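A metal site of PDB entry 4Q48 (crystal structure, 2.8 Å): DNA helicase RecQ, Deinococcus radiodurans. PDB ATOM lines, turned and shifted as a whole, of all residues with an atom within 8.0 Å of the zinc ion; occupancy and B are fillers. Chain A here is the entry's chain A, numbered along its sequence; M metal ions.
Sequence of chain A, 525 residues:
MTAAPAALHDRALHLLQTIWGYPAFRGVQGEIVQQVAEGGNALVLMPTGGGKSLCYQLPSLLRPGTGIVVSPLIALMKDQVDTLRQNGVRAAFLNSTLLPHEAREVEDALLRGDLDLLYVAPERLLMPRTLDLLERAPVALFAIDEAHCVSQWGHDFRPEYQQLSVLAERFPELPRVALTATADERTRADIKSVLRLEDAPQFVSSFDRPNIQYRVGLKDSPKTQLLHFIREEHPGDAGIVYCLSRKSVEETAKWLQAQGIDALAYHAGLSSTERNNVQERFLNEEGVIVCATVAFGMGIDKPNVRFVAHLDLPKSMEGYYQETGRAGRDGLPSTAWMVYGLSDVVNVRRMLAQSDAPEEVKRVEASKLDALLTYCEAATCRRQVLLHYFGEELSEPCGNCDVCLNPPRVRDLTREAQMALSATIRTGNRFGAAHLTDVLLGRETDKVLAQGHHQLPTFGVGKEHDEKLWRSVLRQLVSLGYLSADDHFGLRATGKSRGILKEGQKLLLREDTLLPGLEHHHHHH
The side-chain sulfur of Cys 381 lies close to the backbone NH of Arg 383, at 3.6 Å. N of Gly 399 lies close to SG of Cys 404 (3.3 Å). The side-chain sulfur (SG) of Cys 398 lies close to the backbone NH (N) of Asn 400 (3.1 Å). The side-chain sulfur of Cys 401 sits close to the backbone NH of Arg 382 (3.4 Å). The side-chain sulfur (SG) of Cys 381 sits close to the backbone NH (N) of Gln 384, at 3.6 Å. The backbone NH of Val 403 lies close to the side-chain sulfur of Cys 401. The side-chain sulfur (SG) of Cys 398 lies close to the guanidinium group (NE) of Arg 383.
Residues that only touch the zinc ion: Gly 399 (3.7 Å).
The zinc ion is bound by SG of Cys 401 (2.3 Å), SG of Cys 381 (2.4 Å), SG of Cys 398 (2.4 Å) and SG of Cys 404 (2.4 Å). The zinc ion has four donor atoms within binding distance.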
ATOM      1  N   TYR A 214      17.221  13.746  -1.166  1.00  0.00           N
ATOM      2  CA  TYR A 214      17.868  13.679   0.174  1.00  0.00           C
ATOM      3  C   TYR A 214      19.343  13.228   0.131  1.00  0.00           C
ATOM      4  O   TYR A 214      19.685  12.237  -0.527  1.00  0.00           O
ATOM      5  CB  TYR A 214      17.077  12.769   1.115  1.00  0.00           C
ATOM      6  CG  TYR A 214      15.690  13.300   1.413  1.00  0.00           C
ATOM      7  CD1 TYR A 214      15.476  14.187   2.464  1.00  0.00           C
ATOM      8  CD2 TYR A 214      14.622  12.946   0.600  1.00  0.00           C
ATOM      9  CE1 TYR A 214      14.200  14.681   2.713  1.00  0.00           C
ATOM     10  CE2 TYR A 214      13.362  13.456   0.827  1.00  0.00           C
ATOM     11  CZ  TYR A 214      13.145  14.315   1.887  1.00  0.00           C
ATOM     12  OH  TYR A 214      11.878  14.782   2.082  1.00  0.00           O
ATOM     13  N   THR A 380      20.667   1.206   2.205  1.00  0.00           N
ATOM     14  CA  THR A 380      19.697   1.224   1.126  1.00  0.00           C
ATOM     15  C   THR A 380      18.970   2.548   1.187  1.00  0.00           C
ATOM     16  O   THR A 380      19.042   3.234   2.201  1.00  0.00           O
ATOM     17  CB  THR A 380      18.699   0.034   1.250  1.00  0.00           C
ATOM     18  OG1 THR A 380      18.122   0.016   2.581  1.00  0.00           O
ATOM     19  CG2 THR A 380      19.443  -1.287   1.031  1.00  0.00           C
ATOM     20  N   CYS A 381      18.278   2.883   0.116  1.00  0.00           N
ATOM     21  CA  CYS A 381      17.504   4.142  -0.041  1.00  0.00           C
ATOM     22  C   CYS A 381      17.186   4.910   1.233  1.00  0.00           C
ATOM     23  O   CYS A 381      16.530   4.363   2.126  1.00  0.00           O
ATOM     24  CB  CYS A 381      16.203   3.805  -0.765  1.00  0.00           C
ATOM     25  SG  CYS A 381      15.121   5.190  -1.137  1.00  0.00           S
ATOM     26  N   ARG A 382      17.658   6.157   1.341  1.00  0.00           N
ATOM     27  CA  ARG A 382      17.386   6.972   2.524  1.00  0.00           C
ATOM     28  C   ARG A 382      15.906   7.262   2.698  1.00  0.00           C
ATOM     29  O   ARG A 382      15.425   7.322   3.816  1.00  0.00           O
ATOM     30  CB  ARG A 382      18.066   8.332   2.482  1.00  0.00           C
ATOM     31  CG  ARG A 382      19.451   8.350   2.035  1.00  0.00           C
ATOM     32  CD  ARG A 382      20.053   9.605   2.541  1.00  0.00           C
ATOM     33  NE  ARG A 382      20.645   9.268   3.811  1.00  0.00           N
ATOM     34  CZ  ARG A 382      21.870   8.805   3.928  1.00  0.00           C
ATOM     35  NH1 ARG A 382      22.629   8.685   2.832  1.00  0.00           N
ATOM     36  NH2 ARG A 382      22.342   8.497   5.119  1.00  0.00           N
ATOM     37  N   ARG A 383      15.223   7.517   1.584  1.00  0.00           N
ATOM     38  CA  ARG A 383      13.840   7.969   1.606  1.00  0.00           C
ATOM     39  C   ARG A 383      12.979   6.887   2.254  1.00  0.00           C
ATOM     40  O   ARG A 383      12.224   7.174   3.182  1.00  0.00           O
ATOM     41  CB  ARG A 383      13.331   8.285   0.197  1.00  0.00           C
ATOM     42  CG  ARG A 383      12.126   9.220   0.143  1.00  0.00           C
ATOM     43  CD  ARG A 383      11.651   9.492  -1.254  1.00  0.00           C
ATOM     44  NE  ARG A 383      12.622  10.233  -2.033  1.00  0.00           N
ATOM     45  CZ  ARG A 383      12.635  11.557  -2.151  1.00  0.00           C
ATOM     46  NH1 ARG A 383      11.701  12.265  -1.540  1.00  0.00           N
ATOM     47  NH2 ARG A 383      13.565  12.163  -2.894  1.00  0.00           N
ATOM     48  N   GLN A 384      13.157   5.633   1.841  1.00  0.00           N
ATOM     49  CA  GLN A 384      12.457   4.511   2.453  1.00  0.00           C
ATOM     50  C   GLN A 384      12.624   4.503   3.975  1.00  0.00           C
ATOM     51  O   GLN A 384      11.634   4.344   4.694  1.00  0.00           O
ATOM     52  CB  GLN A 384      12.938   3.174   1.891  1.00  0.00           C
ATOM     53  CG  GLN A 384      12.309   2.803   0.559  1.00  0.00           C
ATOM     54  CD  GLN A 384      12.891   1.533  -0.053  1.00  0.00           C
ATOM     55  OE1 GLN A 384      14.046   1.167   0.173  1.00  0.00           O
ATOM     56  NE2 GLN A 384      12.078   0.855  -0.860  1.00  0.00           N
ATOM     57  N   VAL A 385      13.843   4.705   4.465  1.00  0.00           N
ATOM     58  CA  VAL A 385      14.077   4.700   5.906  1.00  0.00           C
ATOM     59  C   VAL A 385      13.377   5.852   6.595  1.00  0.00           C
ATOM     60  O   VAL A 385      12.801   5.674   7.672  1.00  0.00           O
ATOM     61  CB  VAL A 385      15.586   4.741   6.236  1.00  0.00           C
ATOM     62  CG1 VAL A 385      15.823   5.091   7.707  1.00  0.00           C
ATOM     63  CG2 VAL A 385      16.275   3.414   5.863  1.00  0.00           C
ATOM     64  N   LEU A 394       7.434   2.832   1.583  1.00  0.00           N
ATOM     65  CA  LEU A 394       7.607   3.054   0.148  1.00  0.00           C
ATOM     66  C   LEU A 394       8.165   1.798  -0.508  1.00  0.00           C
ATOM     67  O   LEU A 394       9.339   1.484  -0.348  1.00  0.00           O
ATOM     68  CB  LEU A 394       8.542   4.241  -0.097  1.00  0.00           C
ATOM     69  CG  LEU A 394       8.552   4.828  -1.522  1.00  0.00           C
ATOM     70  CD1 LEU A 394       7.312   5.711  -1.721  1.00  0.00           C
ATOM     71  CD2 LEU A 394       9.864   5.542  -1.900  1.00  0.00           C
ATOM     72  N   GLU A 396       9.271   0.583  -3.308  1.00  0.00           N
ATOM     73  CA  GLU A 396      10.444   0.525  -4.156  1.00  0.00           C
ATOM     74  C   GLU A 396      11.397   1.709  -3.837  1.00  0.00           C
ATOM     75  O   GLU A 396      10.948   2.772  -3.402  1.00  0.00           O
ATOM     76  CB  GLU A 396      10.008   0.546  -5.627  1.00  0.00           C
ATOM     77  CG  GLU A 396       9.043  -0.597  -5.991  1.00  0.00           C
ATOM     78  CD  GLU A 396       9.672  -1.994  -5.940  1.00  0.00           C
ATOM     79  OE1 GLU A 396      10.569  -2.293  -6.763  1.00  0.00           O
ATOM     80  OE2 GLU A 396       9.268  -2.788  -5.056  1.00  0.00           O
ATOM     81  N   PRO A 397      12.721   1.494  -3.995  1.00  0.00           N
ATOM     82  CA  PRO A 397      13.730   2.552  -3.874  1.00  0.00           C
ATOM     83  C   PRO A 397      13.352   3.783  -4.689  1.00  0.00           C
ATOM     84  O   PRO A 397      12.778   3.634  -5.766  1.00  0.00           O
ATOM     85  CB  PRO A 397      14.989   1.889  -4.394  1.00  0.00           C
ATOM     86  CG  PRO A 397      14.800   0.448  -4.100  1.00  0.00           C
ATOM     87  CD  PRO A 397      13.340   0.164  -4.128  1.00  0.00           C
ATOM     88  N   CYS A 398      13.665   4.967  -4.180  1.00  0.00           N
ATOM     89  CA  CYS A 398      13.133   6.180  -4.794  1.00  0.00           C
ATOM     90  C   CYS A 398      13.884   6.648  -6.050  1.00  0.00           C
ATOM     91  O   CYS A 398      13.268   7.118  -7.001  1.00  0.00           O
ATOM     92  CB  CYS A 398      13.101   7.322  -3.781  1.00  0.00           C
ATOM     93  SG  CYS A 398      14.725   8.009  -3.406  1.00  0.00           S
ATOM     94  N   GLY A 399      15.214   6.496  -6.078  1.00  0.00           N
ATOM     95  CA  GLY A 399      15.954   6.957  -7.234  1.00  0.00           C
ATOM     96  C   GLY A 399      16.241   8.454  -7.197  1.00  0.00           C
ATOM     97  O   GLY A 399      16.664   9.048  -8.179  1.00  0.00           O
ATOM     98  N   ASN A 400      15.961   9.081  -6.059  1.00  0.00           N
ATOM     99  CA  ASN A 400      16.269  10.483  -5.893  1.00  0.00           C
ATOM    100  C   ASN A 400      16.864  10.740  -4.514  1.00  0.00           C
ATOM    101  O   ASN A 400      16.559  11.732  -3.860  1.00  0.00           O
ATOM    102  CB  ASN A 400      15.025  11.338  -6.084  1.00  0.00           C
ATOM    103  CG  ASN A 400      15.363  12.764  -6.450  1.00  0.00           C
ATOM    104  OD1 ASN A 400      16.306  13.008  -7.225  1.00  0.00           O
ATOM    105  ND2 ASN A 400      14.612  13.735  -5.888  1.00  0.00           N
ATOM    106  N   CYS A 401      17.758   9.852  -4.089  1.00  0.00           N
ATOM    107  CA  CYS A 401      18.525  10.113  -2.874  1.00  0.00           C
ATOM    108  C   CYS A 401      19.976   9.703  -3.124  1.00  0.00           C
ATOM    109  O   CYS A 401      20.253   8.976  -4.089  1.00  0.00           O
ATOM    110  CB  CYS A 401      17.925   9.389  -1.667  1.00  0.00           C
ATOM    111  SG  CYS A 401      18.203   7.640  -1.666  1.00  0.00           S
ATOM    112  N   ASP A 402      20.890  10.221  -2.311  1.00  0.00           N
ATOM    113  CA  ASP A 402      22.303   9.940  -2.561  1.00  0.00           C
ATOM    114  C   ASP A 402      22.627   8.457  -2.444  1.00  0.00           C
ATOM    115  O   ASP A 402      23.490   7.977  -3.158  1.00  0.00           O
ATOM    116  CB  ASP A 402      23.184  10.768  -1.649  1.00  0.00           C
ATOM    117  CG  ASP A 402      22.932  10.510  -0.187  1.00  0.00           C
ATOM    118  OD1 ASP A 402      21.962   9.777   0.146  1.00  0.00           O
ATOM    119  OD2 ASP A 402      23.690  11.079   0.620  1.00  0.00           O
ATOM    120  N   VAL A 403      21.943   7.731  -1.577  1.00  0.00           N
ATOM    121  CA  VAL A 403      22.169   6.292  -1.488  1.00  0.00           C
ATOM    122  C   VAL A 403      21.744   5.581  -2.763  1.00  0.00           C
ATOM    123  O   VAL A 403      22.494   4.741  -3.287  1.00  0.00           O
ATOM    124  CB  VAL A 403      21.394   5.695  -0.287  1.00  0.00           C
ATOM    125  CG1 VAL A 403      21.340   4.169  -0.364  1.00  0.00           C
ATOM    126  CG2 VAL A 403      21.999   6.172   1.026  1.00  0.00           C
ATOM    127  N   CYS A 404      20.553   5.921  -3.256  1.00  0.00           N
ATOM    128  CA  CYS A 404      20.007   5.355  -4.498  1.00  0.00           C
ATOM    129  C   CYS A 404      20.920   5.650  -5.709  1.00  0.00           C
ATOM    130  O   CYS A 404      21.182   4.766  -6.535  1.00  0.00           O
ATOM    131  CB  CYS A 404      18.600   5.898  -4.761  1.00  0.00           C
ATOM    132  SG  CYS A 404      17.292   4.918  -4.130  1.00  0.00           S
ATOM    133  N   LEU A 405      21.396   6.896  -5.802  1.00  0.00           N
ATOM    134  CA  LEU A 405      22.136   7.357  -6.959  1.00  0.00           C
ATOM    135  C   LEU A 405      23.612   6.978  -6.891  1.00  0.00           C
ATOM    136  O   LEU A 405      24.265   6.742  -7.907  1.00  0.00           O
ATOM    137  CB  LEU A 405      21.998   8.896  -7.106  1.00  0.00           C
ATOM    138  CG  LEU A 405      20.607   9.494  -7.353  1.00  0.00           C
ATOM    139  CD1 LEU A 405      20.580  11.025  -7.171  1.00  0.00           C
ATOM    140  CD2 LEU A 405      20.081   9.091  -8.723  1.00  0.00           C
HETATM  141 ZN    ZN M   1      16.410   6.530  -2.601  1.00  0.00          ZN
